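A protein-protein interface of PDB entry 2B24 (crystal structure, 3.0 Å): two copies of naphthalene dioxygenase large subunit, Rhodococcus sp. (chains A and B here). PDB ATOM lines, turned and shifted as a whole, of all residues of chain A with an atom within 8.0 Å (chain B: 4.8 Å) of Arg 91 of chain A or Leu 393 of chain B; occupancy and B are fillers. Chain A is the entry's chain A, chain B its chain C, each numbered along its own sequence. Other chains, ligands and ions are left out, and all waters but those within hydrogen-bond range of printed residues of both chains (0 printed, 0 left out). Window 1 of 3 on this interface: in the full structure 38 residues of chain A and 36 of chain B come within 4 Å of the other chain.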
ATOM      1  N   ALA A  87     -21.110  27.038  31.697  1.00  0.00           N
ATOM      2  CA  ALA A  87     -20.830  25.868  30.872  1.00  0.00           C
ATOM      3  C   ALA A  87     -19.401  25.394  31.120  1.00  0.00           C
ATOM      4  O   ALA A  87     -18.444  26.132  30.869  1.00  0.00           O
ATOM      5  CB  ALA A  87     -21.045  26.193  29.400  1.00  0.00           C
ATOM      6  N   CYS A  88     -19.271  24.175  31.631  1.00  0.00           N
ATOM      7  CA  CYS A  88     -17.976  23.564  31.921  1.00  0.00           C
ATOM      8  C   CYS A  88     -17.038  23.680  30.733  1.00  0.00           C
ATOM      9  O   CYS A  88     -17.488  23.822  29.595  1.00  0.00           O
ATOM     10  CB  CYS A  88     -18.169  22.085  32.267  1.00  0.00           C
ATOM     11  SG  CYS A  88     -16.743  21.290  33.024  1.00  0.00           S
ATOM     12  N   ARG A  89     -15.734  23.619  30.991  1.00  0.00           N
ATOM     13  CA  ARG A  89     -14.757  23.740  29.914  1.00  0.00           C
ATOM     14  C   ARG A  89     -14.529  22.377  29.259  1.00  0.00           C
ATOM     15  O   ARG A  89     -14.170  22.286  28.097  1.00  0.00           O
ATOM     16  CB  ARG A  89     -13.444  24.361  30.417  1.00  0.00           C
ATOM     17  CG  ARG A  89     -13.508  25.837  30.805  1.00  0.00           C
ATOM     18  CD  ARG A  89     -14.019  26.761  29.712  1.00  0.00           C
ATOM     19  NE  ARG A  89     -12.982  27.599  29.103  1.00  0.00           N
ATOM     20  CZ  ARG A  89     -12.596  27.506  27.835  1.00  0.00           C
ATOM     21  NH1 ARG A  89     -13.132  26.598  27.019  1.00  0.00           N
ATOM     22  NH2 ARG A  89     -11.662  28.316  27.383  1.00  0.00           N
ATOM     23  N   HIS A  90     -14.767  21.322  30.013  1.00  0.00           N
ATOM     24  CA  HIS A  90     -14.617  19.962  29.504  1.00  0.00           C
ATOM     25  C   HIS A  90     -15.609  19.618  28.382  1.00  0.00           C
ATOM     26  O   HIS A  90     -15.233  19.593  27.213  1.00  0.00           O
ATOM     27  CB  HIS A  90     -14.723  18.934  30.642  1.00  0.00           C
ATOM     28  CG  HIS A  90     -14.298  17.563  30.245  1.00  0.00           C
ATOM     29  ND1 HIS A  90     -14.852  16.429  30.787  1.00  0.00           N
ATOM     30  CD2 HIS A  90     -13.368  17.140  29.357  1.00  0.00           C
ATOM     31  CE1 HIS A  90     -14.280  15.364  30.255  1.00  0.00           C
ATOM     32  NE2 HIS A  90     -13.378  15.767  29.380  1.00  0.00           N
ATOM     33  N   ARG A  91     -16.863  19.345  28.758  1.00  0.00           N
ATOM     34  CA  ARG A  91     -17.918  19.004  27.804  1.00  0.00           C
ATOM     35  C   ARG A  91     -19.117  19.932  27.844  1.00  0.00           C
ATOM     36  O   ARG A  91     -20.117  19.650  27.211  1.00  0.00           O
ATOM     37  CB  ARG A  91     -18.397  17.564  27.993  1.00  0.00           C
ATOM     38  CG  ARG A  91     -18.924  16.941  26.719  1.00  0.00           C
ATOM     39  CD  ARG A  91     -17.827  16.478  25.741  1.00  0.00           C
ATOM     40  NE  ARG A  91     -17.377  15.128  26.062  1.00  0.00           N
ATOM     41  CZ  ARG A  91     -16.176  14.828  26.533  1.00  0.00           C
ATOM     42  NH1 ARG A  91     -15.265  15.782  26.723  1.00  0.00           N
ATOM     43  NH2 ARG A  91     -15.880  13.562  26.807  1.00  0.00           N
ATOM     44  N   GLY A  92     -19.028  21.027  28.587  1.00  0.00           N
ATOM     45  CA  GLY A  92     -20.040  22.069  28.512  1.00  0.00           C
ATOM     46  C   GLY A  92     -21.304  21.815  29.312  1.00  0.00           C
ATOM     47  O   GLY A  92     -22.379  22.244  28.936  1.00  0.00           O
ATOM     48  N   MET A  93     -21.177  21.119  30.425  1.00  0.00           N
ATOM     49  CA  MET A  93     -22.297  20.903  31.324  1.00  0.00           C
ATOM     50  C   MET A  93     -22.514  22.113  32.223  1.00  0.00           C
ATOM     51  O   MET A  93     -21.594  22.887  32.451  1.00  0.00           O
ATOM     52  CB  MET A  93     -22.048  19.646  32.155  1.00  0.00           C
ATOM     53  CG  MET A  93     -22.769  19.603  33.463  1.00  0.00           C
ATOM     54  SD  MET A  93     -23.609  18.062  33.726  1.00  0.00           S
ATOM     55  CE  MET A  93     -24.955  18.658  34.773  1.00  0.00           C
ATOM     56  N   GLN A  94     -23.743  22.277  32.711  1.00  0.00           N
ATOM     57  CA  GLN A  94     -24.046  23.302  33.699  1.00  0.00           C
ATOM     58  C   GLN A  94     -23.233  22.973  34.945  1.00  0.00           C
ATOM     59  O   GLN A  94     -23.390  21.903  35.546  1.00  0.00           O
ATOM     60  CB  GLN A  94     -25.545  23.345  34.030  1.00  0.00           C
ATOM     61  CG  GLN A  94     -26.403  24.091  33.024  1.00  0.00           C
ATOM     62  CD  GLN A  94     -27.889  23.969  33.304  1.00  0.00           C
ATOM     63  OE1 GLN A  94     -28.413  22.864  33.467  1.00  0.00           O
ATOM     64  NE2 GLN A  94     -28.573  25.104  33.353  1.00  0.00           N
ATOM     65  N   CYS A 108     -18.573  20.332  38.801  1.00  0.00           N
ATOM     66  CA  CYS A 108     -19.341  19.896  37.628  1.00  0.00           C
ATOM     67  C   CYS A 108     -19.735  18.440  37.787  1.00  0.00           C
ATOM     68  O   CYS A 108     -18.883  17.612  38.063  1.00  0.00           O
ATOM     69  CB  CYS A 108     -18.532  20.091  36.334  1.00  0.00           C
ATOM     70  SG  CYS A 108     -19.151  19.205  34.876  1.00  0.00           S
ATOM     71  N   TYR A 110     -20.743  16.069  35.631  1.00  0.00           N
ATOM     72  CA  TYR A 110     -20.369  15.089  34.602  1.00  0.00           C
ATOM     73  C   TYR A 110     -19.092  14.344  34.989  1.00  0.00           C
ATOM     74  O   TYR A 110     -19.160  13.179  35.380  1.00  0.00           O
ATOM     75  CB  TYR A 110     -20.220  15.759  33.217  1.00  0.00           C
ATOM     76  CG  TYR A 110     -20.545  14.900  31.988  1.00  0.00           C
ATOM     77  CD1 TYR A 110     -20.657  15.498  30.737  1.00  0.00           C
ATOM     78  CD2 TYR A 110     -20.712  13.509  32.066  1.00  0.00           C
ATOM     79  CE1 TYR A 110     -20.932  14.756  29.593  1.00  0.00           C
ATOM     80  CE2 TYR A 110     -20.988  12.743  30.912  1.00  0.00           C
ATOM     81  CZ  TYR A 110     -21.103  13.382  29.675  1.00  0.00           C
ATOM     82  OH  TYR A 110     -21.381  12.679  28.509  1.00  0.00           O
ATOM     83  N   HIS A 111     -17.936  15.007  34.903  1.00  0.00           N
ATOM     84  CA  HIS A 111     -16.660  14.324  35.169  1.00  0.00           C
ATOM     85  C   HIS A 111     -16.010  14.663  36.523  1.00  0.00           C
ATOM     86  O   HIS A 111     -15.267  13.849  37.087  1.00  0.00           O
ATOM     87  CB  HIS A 111     -15.682  14.526  34.011  1.00  0.00           C
ATOM     88  CG  HIS A 111     -16.207  14.046  32.697  1.00  0.00           C
ATOM     89  ND1 HIS A 111     -16.872  14.871  31.822  1.00  0.00           N
ATOM     90  CD2 HIS A 111     -16.184  12.824  32.115  1.00  0.00           C
ATOM     91  CE1 HIS A 111     -17.225  14.185  30.750  1.00  0.00           C
ATOM     92  NE2 HIS A 111     -16.818  12.938  30.902  1.00  0.00           N
ATOM     93  N   TRP A 113     -14.732  18.085  37.323  1.00  0.00           N
ATOM     94  CA  TRP A 113     -13.873  19.265  37.307  1.00  0.00           C
ATOM     95  C   TRP A 113     -14.406  20.295  38.305  1.00  0.00           C
ATOM     96  O   TRP A 113     -15.494  20.825  38.109  1.00  0.00           O
ATOM     97  CB  TRP A 113     -13.812  19.883  35.906  1.00  0.00           C
ATOM     98  CG  TRP A 113     -12.985  19.144  34.893  1.00  0.00           C
ATOM     99  CD1 TRP A 113     -12.693  17.817  34.872  1.00  0.00           C
ATOM    100  CD2 TRP A 113     -12.365  19.704  33.740  1.00  0.00           C
ATOM    101  NE1 TRP A 113     -11.923  17.511  33.778  1.00  0.00           N
ATOM    102  CE2 TRP A 113     -11.707  18.657  33.063  1.00  0.00           C
ATOM    103  CE3 TRP A 113     -12.291  20.996  33.202  1.00  0.00           C
ATOM    104  CZ2 TRP A 113     -10.984  18.859  31.881  1.00  0.00           C
ATOM    105  CZ3 TRP A 113     -11.578  21.193  32.022  1.00  0.00           C
ATOM    106  CH2 TRP A 113     -10.935  20.129  31.377  1.00  0.00           C
ATOM    107  N   TYR A 115     -14.400  23.892  40.153  1.00  0.00           N
ATOM    108  CA  TYR A 115     -14.014  25.271  39.918  1.00  0.00           C
ATOM    109  C   TYR A 115     -14.208  26.052  41.218  1.00  0.00           C
ATOM    110  O   TYR A 115     -15.112  25.755  41.990  1.00  0.00           O
ATOM    111  CB  TYR A 115     -14.916  25.874  38.850  1.00  0.00           C
ATOM    112  CG  TYR A 115     -14.806  25.245  37.477  1.00  0.00           C
ATOM    113  CD1 TYR A 115     -15.326  23.972  37.219  1.00  0.00           C
ATOM    114  CD2 TYR A 115     -14.205  25.939  36.426  1.00  0.00           C
ATOM    115  CE1 TYR A 115     -15.228  23.408  35.952  1.00  0.00           C
ATOM    116  CE2 TYR A 115     -14.106  25.385  35.164  1.00  0.00           C
ATOM    117  CZ  TYR A 115     -14.618  24.123  34.933  1.00  0.00           C
ATOM    118  OH  TYR A 115     -14.526  23.566  33.681  1.00  0.00           O
ATOM    119  N   TYR A 131      -4.846  12.244  32.729  1.00  0.00           N
ATOM    120  CA  TYR A 131      -4.151  13.288  31.970  1.00  0.00           C
ATOM    121  C   TYR A 131      -2.635  13.238  32.102  1.00  0.00           C
ATOM    122  O   TYR A 131      -1.924  13.873  31.313  1.00  0.00           O
ATOM    123  CB  TYR A 131      -4.631  14.675  32.414  1.00  0.00           C
ATOM    124  CG  TYR A 131      -6.075  14.988  32.075  1.00  0.00           C
ATOM    125  CD1 TYR A 131      -7.110  14.556  32.902  1.00  0.00           C
ATOM    126  CD2 TYR A 131      -6.406  15.717  30.925  1.00  0.00           C
ATOM    127  CE1 TYR A 131      -8.437  14.836  32.598  1.00  0.00           C
ATOM    128  CE2 TYR A 131      -7.735  16.005  30.618  1.00  0.00           C
ATOM    129  CZ  TYR A 131      -8.742  15.561  31.465  1.00  0.00           C
ATOM    130  OH  TYR A 131     -10.060  15.830  31.182  1.00  0.00           O
ATOM    131  N   TRP A 140      -8.193  26.614  31.235  1.00  0.00           N
ATOM    132  CA  TRP A 140      -9.527  26.021  31.216  1.00  0.00           C
ATOM    133  C   TRP A 140     -10.395  26.521  32.372  1.00  0.00           C
ATOM    134  O   TRP A 140     -10.963  25.732  33.129  1.00  0.00           O
ATOM    135  CB  TRP A 140      -9.422  24.489  31.209  1.00  0.00           C
ATOM    136  CG  TRP A 140      -8.467  23.982  30.170  1.00  0.00           C
ATOM    137  CD1 TRP A 140      -7.243  23.404  30.387  1.00  0.00           C
ATOM    138  CD2 TRP A 140      -8.641  24.016  28.746  1.00  0.00           C
ATOM    139  NE1 TRP A 140      -6.652  23.066  29.191  1.00  0.00           N
ATOM    140  CE2 TRP A 140      -7.484  23.433  28.165  1.00  0.00           C
ATOM    141  CE3 TRP A 140      -9.658  24.477  27.896  1.00  0.00           C
ATOM    142  CZ2 TRP A 140      -7.318  23.308  26.780  1.00  0.00           C
ATOM    143  CZ3 TRP A 140      -9.493  24.346  26.518  1.00  0.00           C
ATOM    144  CH2 TRP A 140      -8.330  23.766  25.975  1.00  0.00           C
ATOM    145  N   TRP B  21      -6.648  19.161  20.104  1.00  0.00           N
ATOM    146  CA  TRP B  21      -7.513  18.170  20.756  1.00  0.00           C
ATOM    147  C   TRP B  21      -8.738  18.802  21.426  1.00  0.00           C
ATOM    148  O   TRP B  21      -9.104  18.454  22.541  1.00  0.00           O
ATOM    149  CB  TRP B  21      -6.728  17.267  21.722  1.00  0.00           C
ATOM    150  CG  TRP B  21      -5.817  16.280  21.034  1.00  0.00           C
ATOM    151  CD1 TRP B  21      -5.378  16.324  19.734  1.00  0.00           C
ATOM    152  CD2 TRP B  21      -5.225  15.106  21.610  1.00  0.00           C
ATOM    153  NE1 TRP B  21      -4.563  15.248  19.470  1.00  0.00           N
ATOM    154  CE2 TRP B  21      -4.447  14.486  20.601  1.00  0.00           C
ATOM    155  CE3 TRP B  21      -5.276  14.512  22.875  1.00  0.00           C
ATOM    156  CZ2 TRP B  21      -3.734  13.313  20.817  1.00  0.00           C
ATOM    157  CZ3 TRP B  21      -4.566  13.338  23.088  1.00  0.00           C
ATOM    158  CH2 TRP B  21      -3.797  12.758  22.065  1.00  0.00           C
ATOM    159  N   THR B  22      -9.354  19.746  20.724  1.00  0.00           N
ATOM    160  CA  THR B  22     -10.657  20.270  21.083  1.00  0.00           C
ATOM    161  C   THR B  22     -11.600  20.154  19.873  1.00  0.00           C
ATOM    162  O   THR B  22     -11.180  19.779  18.775  1.00  0.00           O
ATOM    163  CB  THR B  22     -10.563  21.742  21.488  1.00  0.00           C
ATOM    164  OG1 THR B  22     -10.344  22.525  20.314  1.00  0.00           O
ATOM    165  CG2 THR B  22      -9.335  22.033  22.305  1.00  0.00           C
ATOM    166  N   VAL B  23     -12.873  20.486  20.080  1.00  0.00           N
ATOM    167  CA  VAL B  23     -13.876  20.476  19.018  1.00  0.00           C
ATOM    168  C   VAL B  23     -14.777  21.701  19.233  1.00  0.00           C
ATOM    169  O   VAL B  23     -15.054  22.049  20.375  1.00  0.00           O
ATOM    170  CB  VAL B  23     -14.695  19.146  19.041  1.00  0.00           C
ATOM    171  CG1 VAL B  23     -15.773  19.126  17.947  1.00  0.00           C
ATOM    172  CG2 VAL B  23     -13.774  17.932  18.910  1.00  0.00           C
ATOM    173  N   PRO B  24     -15.222  22.364  18.164  1.00  0.00           N
ATOM    174  CA  PRO B  24     -16.076  23.548  18.318  1.00  0.00           C
ATOM    175  C   PRO B  24     -17.372  23.145  18.999  1.00  0.00           C
ATOM    176  O   PRO B  24     -17.940  22.112  18.632  1.00  0.00           O
ATOM    177  CB  PRO B  24     -16.342  23.997  16.870  1.00  0.00           C
ATOM    178  CG  PRO B  24     -15.307  23.335  16.053  1.00  0.00           C
ATOM    179  CD  PRO B  24     -14.970  22.049  16.748  1.00  0.00           C
ATOM    180  N   ALA B  25     -17.816  23.931  19.976  1.00  0.00           N
ATOM    181  CA  ALA B  25     -19.025  23.606  20.740  1.00  0.00           C
ATOM    182  C   ALA B  25     -20.320  23.821  19.949  1.00  0.00           C
ATOM    183  O   ALA B  25     -21.357  23.270  20.316  1.00  0.00           O
ATOM    184  CB  ALA B  25     -19.064  24.380  22.060  1.00  0.00           C
ATOM    185  N   ILE B  28     -23.272  21.054  18.948  1.00  0.00           N
ATOM    186  CA  ILE B  28     -24.204  20.317  19.804  1.00  0.00           C
ATOM    187  C   ILE B  28     -25.653  20.748  19.650  1.00  0.00           C
ATOM    188  O   ILE B  28     -26.509  19.889  19.411  1.00  0.00           O
ATOM    189  CB  ILE B  28     -23.774  20.320  21.280  1.00  0.00           C
ATOM    190  CG1 ILE B  28     -22.347  19.777  21.398  1.00  0.00           C
ATOM    191  CG2 ILE B  28     -24.740  19.487  22.117  1.00  0.00           C
ATOM    192  CD1 ILE B  28     -21.950  19.313  22.773  1.00  0.00           C
ATOM    193  N   LEU B 205     -24.479  13.486  22.430  1.00  0.00           N
ATOM    194  CA  LEU B 205     -23.982  13.532  23.800  1.00  0.00           C
ATOM    195  C   LEU B 205     -24.050  12.168  24.451  1.00  0.00           C
ATOM    196  O   LEU B 205     -23.220  11.829  25.300  1.00  0.00           O
ATOM    197  CB  LEU B 205     -24.769  14.546  24.623  1.00  0.00           C
ATOM    198  CG  LEU B 205     -24.519  16.006  24.267  1.00  0.00           C
ATOM    199  CD1 LEU B 205     -25.706  16.810  24.643  1.00  0.00           C
ATOM    200  CD2 LEU B 205     -23.312  16.538  24.978  1.00  0.00           C
ATOM    201  N   ASP B 208     -21.413  10.167  22.219  1.00  0.00           N
ATOM    202  CA  ASP B 208     -20.123  10.574  22.769  1.00  0.00           C
ATOM    203  C   ASP B 208     -19.817   9.873  24.086  1.00  0.00           C
ATOM    204  O   ASP B 208     -18.671   9.551  24.345  1.00  0.00           O
ATOM    205  CB  ASP B 208     -20.126  12.086  22.986  1.00  0.00           C
ATOM    206  CG  ASP B 208     -18.819  12.612  23.521  1.00  0.00           C
ATOM    207  OD1 ASP B 208     -18.606  12.532  24.748  1.00  0.00           O
ATOM    208  OD2 ASP B 208     -17.953  13.140  22.791  1.00  0.00           O
ATOM    209  N   ASP B 213     -16.213   7.023  27.230  1.00  0.00           N
ATOM    210  CA  ASP B 213     -16.297   7.777  28.478  1.00  0.00           C
ATOM    211  C   ASP B 213     -16.545   6.852  29.663  1.00  0.00           C
ATOM    212  O   ASP B 213     -17.692   6.626  30.055  1.00  0.00           O
ATOM    213  CB  ASP B 213     -17.359   8.873  28.396  1.00  0.00           C
ATOM    214  CG  ASP B 213     -16.971  10.126  29.155  1.00  0.00           C
ATOM    215  OD1 ASP B 213     -16.863  10.037  30.394  1.00  0.00           O
ATOM    216  OD2 ASP B 213     -16.771  11.238  28.604  1.00  0.00           O
ATOM    217  N   ILE B 379     -26.260  19.971  29.361  1.00  0.00           N
ATOM    218  CA  ILE B 379     -25.213  20.384  28.435  1.00  0.00           C
ATOM    219  C   ILE B 379     -25.891  21.055  27.259  1.00  0.00           C
ATOM    220  O   ILE B 379     -25.553  22.178  26.898  1.00  0.00           O
ATOM    221  CB  ILE B 379     -24.417  19.174  27.942  1.00  0.00           C
ATOM    222  CG1 ILE B 379     -23.569  18.586  29.069  1.00  0.00           C
ATOM    223  CG2 ILE B 379     -23.527  19.557  26.780  1.00  0.00           C
ATOM    224  CD1 ILE B 379     -23.196  17.124  28.878  1.00  0.00           C
ATOM    225  N   GLY B 391     -17.357  28.984  22.153  1.00  0.00           N
ATOM    226  CA  GLY B 391     -16.338  28.179  22.814  1.00  0.00           C
ATOM    227  C   GLY B 391     -16.008  26.844  22.176  1.00  0.00           C
ATOM    228  O   GLY B 391     -16.279  26.630  20.994  1.00  0.00           O
ATOM    229  N   GLU B 392     -15.416  25.948  22.966  1.00  0.00           N
ATOM    230  CA  GLU B 392     -14.979  24.642  22.469  1.00  0.00           C
ATOM    231  C   GLU B 392     -15.040  23.539  23.524  1.00  0.00           C
ATOM    232  O   GLU B 392     -14.861  23.807  24.707  1.00  0.00           O
ATOM    233  CB  GLU B 392     -13.572  24.733  21.854  1.00  0.00           C
ATOM    234  CG  GLU B 392     -12.428  24.832  22.849  1.00  0.00           C
ATOM    235  CD  GLU B 392     -12.360  26.178  23.553  1.00  0.00           C
ATOM    236  OE1 GLU B 392     -12.398  27.224  22.858  1.00  0.00           O
ATOM    237  OE2 GLU B 392     -12.266  26.190  24.803  1.00  0.00           O
ATOM    238  N   LEU B 393     -15.320  22.314  23.081  1.00  0.00           N
ATOM    239  CA  LEU B 393     -15.311  21.136  23.932  1.00  0.00           C
ATOM    240  C   LEU B 393     -13.886  20.637  24.048  1.00  0.00           C
ATOM    241  O   LEU B 393     -13.167  20.592  23.058  1.00  0.00           O
ATOM    242  CB  LEU B 393     -16.153  20.024  23.311  1.00  0.00           C
ATOM    243  CG  LEU B 393     -17.650  20.183  23.035  1.00  0.00           C
ATOM    244  CD1 LEU B 393     -18.175  18.910  22.391  1.00  0.00           C
ATOM    245  CD2 LEU B 393     -18.431  20.498  24.312  1.00  0.00           C
ATOM    246  N   ASN B 394     -13.483  20.247  25.251  1.00  0.00           N
ATOM    247  CA  ASN B 394     -12.110  19.859  25.505  1.00  0.00           C
ATOM    248  C   ASN B 394     -11.963  18.361  25.445  1.00  0.00           C
ATOM    249  O   ASN B 394     -12.581  17.658  26.227  1.00  0.00           O
ATOM    250  CB  ASN B 394     -11.684  20.368  26.874  1.00  0.00           C
ATOM    251  CG  ASN B 394     -10.321  19.878  27.285  1.00  0.00           C
ATOM    252  OD1 ASN B 394     -10.111  18.680  27.468  1.00  0.00           O
ATOM    253  ND2 ASN B 394      -9.386  20.809  27.456  1.00  0.00           N
ATOM    254  N   TYR B 395     -11.137  17.879  24.524  1.00  0.00           N
ATOM    255  CA  TYR B 395     -10.857  16.455  24.396  1.00  0.00           C
ATOM    256  C   TYR B 395      -9.357  16.177  24.475  1.00  0.00           C
ATOM    257  O   TYR B 395      -8.791  15.524  23.592  1.00  0.00           O
ATOM    258  CB  TYR B 395     -11.383  15.949  23.065  1.00  0.00           C
ATOM    259  CG  TYR B 395     -12.874  15.837  22.969  1.00  0.00           C
ATOM    260  CD1 TYR B 395     -13.587  16.692  22.139  1.00  0.00           C
ATOM    261  CD2 TYR B 395     -13.572  14.854  23.672  1.00  0.00           C
ATOM    262  CE1 TYR B 395     -14.968  16.594  22.021  1.00  0.00           C
ATOM    263  CE2 TYR B 395     -14.943  14.737  23.560  1.00  0.00           C
ATOM    264  CZ  TYR B 395     -15.643  15.611  22.733  1.00  0.00           C
ATOM    265  OH  TYR B 395     -17.010  15.505  22.608  1.00  0.00           O
ATOM    266  N   GLU B 421      -9.679   9.899  25.348  1.00  0.00           N
ATOM    267  CA  GLU B 421     -10.760  10.550  24.616  1.00  0.00           C
ATOM    268  C   GLU B 421     -10.408  10.558  23.125  1.00  0.00           C
ATOM    269  O   GLU B 421     -10.829  11.440  22.359  1.00  0.00           O
ATOM    270  CB  GLU B 421     -10.984  11.979  25.140  1.00  0.00           C
ATOM    271  CG  GLU B 421     -11.386  12.059  26.607  1.00  0.00           C
ATOM    272  CD  GLU B 421     -11.631  13.486  27.103  1.00  0.00           C
ATOM    273  OE1 GLU B 421     -10.864  14.408  26.744  1.00  0.00           O
ATOM    274  OE2 GLU B 421     -12.594  13.686  27.879  1.00  0.00           O
ATOM    275  N   GLN B 424     -13.580   9.408  21.194  1.00  0.00           N
ATOM    276  CA  GLN B 424     -14.567  10.462  21.050  1.00  0.00           C
ATOM    277  C   GLN B 424     -14.146  11.444  19.978  1.00  0.00           C
ATOM    278  O   GLN B 424     -15.008  11.982  19.256  1.00  0.00           O
ATOM    279  CB  GLN B 424     -14.738  11.222  22.362  1.00  0.00           C
ATOM    280  CG  GLN B 424     -15.517  10.493  23.408  1.00  0.00           C
ATOM    281  CD  GLN B 424     -14.623   9.964  24.491  1.00  0.00           C
ATOM    282  OE1 GLN B 424     -14.074   8.871  24.360  1.00  0.00           O
ATOM    283  NE2 GLN B 424     -14.468  10.731  25.566  1.00  0.00           N
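The backbone NH (N) of His 90 of chain A lies close to the side-chain sulfur (SG) of Cys 88 of chain A, at 3.6 Å.
The backbone NH (N) of Cys 88 of chain A lies within hydrogen-bond range of the backbone carbonyl oxygen (O) of Met 93 of chain A, 2.8 Å away.
The backbone NH (N) of Arg 89 of chain A lies within hydrogen-bond range of the side-chain hydroxyl (OH) of Tyr 115 of chain A (2.9 Å).
SG of Cys 108 of chain A lies close to N of Tyr 110 of chain A (3.6 Å).
O of Val 23 of chain B sits at hydrogen-bond distance from N of Leu 393 of chain B.
The side-chain hydroxyl (OH) of Tyr 395 of chain B is in hydrogen-bond range of the side-chain carboxylate (OD2) of Asp 208 of chain B.
Printed residues of chain B within 4 Å of Arg 91 of chain A: Asp 208, Asp 213, Ile 379, Leu 393, Asn 394, Tyr 395, Glu 421 and Gln 424.
Leu 393 of chain B touches just these residues of chain A: His 90 and Arg 91.
Printed residues of chain A within 4 Å of Asn 394 of chain B: Arg 89 (3.4 Å), His 90 (2.7 Å), Arg 91 (3.3 Å) and Trp 140 (3.3 Å).
Printed residues of chain A within 4 Å of Asp 208 of chain B: Arg 91 (3.2 Å).
Of the printed residues of chain B, Tyr 110 of chain A touches Leu 205 and Ile 379.
Of the printed residues of chain A, Asp 213 of chain B touches Arg 91 (3.1 Å) and His 111 (2.9 Å).
Trp 21 of chain B touches none of the printed residues of chain A.
Of the 15 printed residues of chain A, 8 touch a printed residue of chain B.
Hydrophobic or aromatic side chains of chain A within 4 Å of the printed part of chain B: His 90, Met 93, Tyr 110, His 111 and Trp 140.
Along chain B the printed residues that touch a printed residue of chain A span positions 205 to 424.
Among the printed residues, 20 pairs touch across the chains.
Among the printed residues, Asp or Glu carboxylates within 4 Å of a Lys or Arg side-chain nitrogen of the other chain: Arg 89 of chain A with Glu 392 of chain B (2.4 Å), Arg 91 of chain A with Asp 208 of chain B (3.2 Å), Arg 91 of chain A with Asp 213 of chain B (3.1 Å) and Arg 91 of chain A with Glu 421 of chain B (3.5 Å).
O of Arg 89 of chain A touches CB of Asn 394 of chain B, 3.4 Å away.
O of His 90 of chain A touches C of Leu 393 of chain B, 3.6 Å away.
CG2 of Ile 379 of chain B touches O of Arg 91 of chain A (3.4 Å).
CD2 of Leu 393 of chain B touches O of Arg 91 of chain A, at 3.5 Å.
O of Gly 92 of chain A touches CA of Ile 379 of chain B, 3.4 Å away.
CG1 of Ile 379 of chain B touches CA of Met 93 of chain A, at 3.5 Å.
O of Leu 205 of chain B touches OH of Tyr 110 of chain A (3.8 Å).
Ile 379 of chain B touches Tyr 110 of chain A.
CZ3 of Trp 140 of chain A touches OE2 of Glu 392 of chain B, 3.7 Å away.
Trp 140 of chain A touches Asn 394 of chain B (CZ2 to ND2, 3.3 Å).
No position is printed for both chains.
NH1 of Arg 89 of chain A lies within salt-bridge range of OE2 of Glu 392 of chain B, at 2.4 Å.
O of His 90 of chain A sits at hydrogen-bond distance from N of Asn 394 of chain B, 2.7 Å away.
A ring nitrogen (NE2) of His 90 of chain A is in hydrogen-bond range of the side-chain carboxylate (OE2) of Glu 421 of chain B, at 2.7 Å.
NE of Arg 91 of chain A lies within salt-bridge range of OD1 of Asp 208 of chain B, at 3.2 Å.
The guanidinium group (NH2) of Arg 91 of chain A is in salt-bridge range of the side-chain carboxylate (OD2) of Asp 213 of chain B.
NH1 of Arg 91 of chain A sits at hydrogen-bond distance from O of Asn 394 of chain B.
The side-chain hydroxyl (OH) of Tyr 395 of chain B sits close to the guanidinium group (NE) of Arg 91 of chain A (3.5 Å).
The guanidinium group (NH2) of Arg 91 of chain A is in salt-bridge range of the side-chain carboxylate (OE2) of Glu 421 of chain B (3.5 Å).
The guanidinium group of Arg 91 of chain A lies close to the side-chain amide nitrogen of Gln 424 of chain B (3.4 Å).
The side-chain carboxylate (OD2) of Asp 213 of chain B is in hydrogen-bond range of a ring nitrogen (NE2) of His 111 of chain A, 2.9 Å away.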
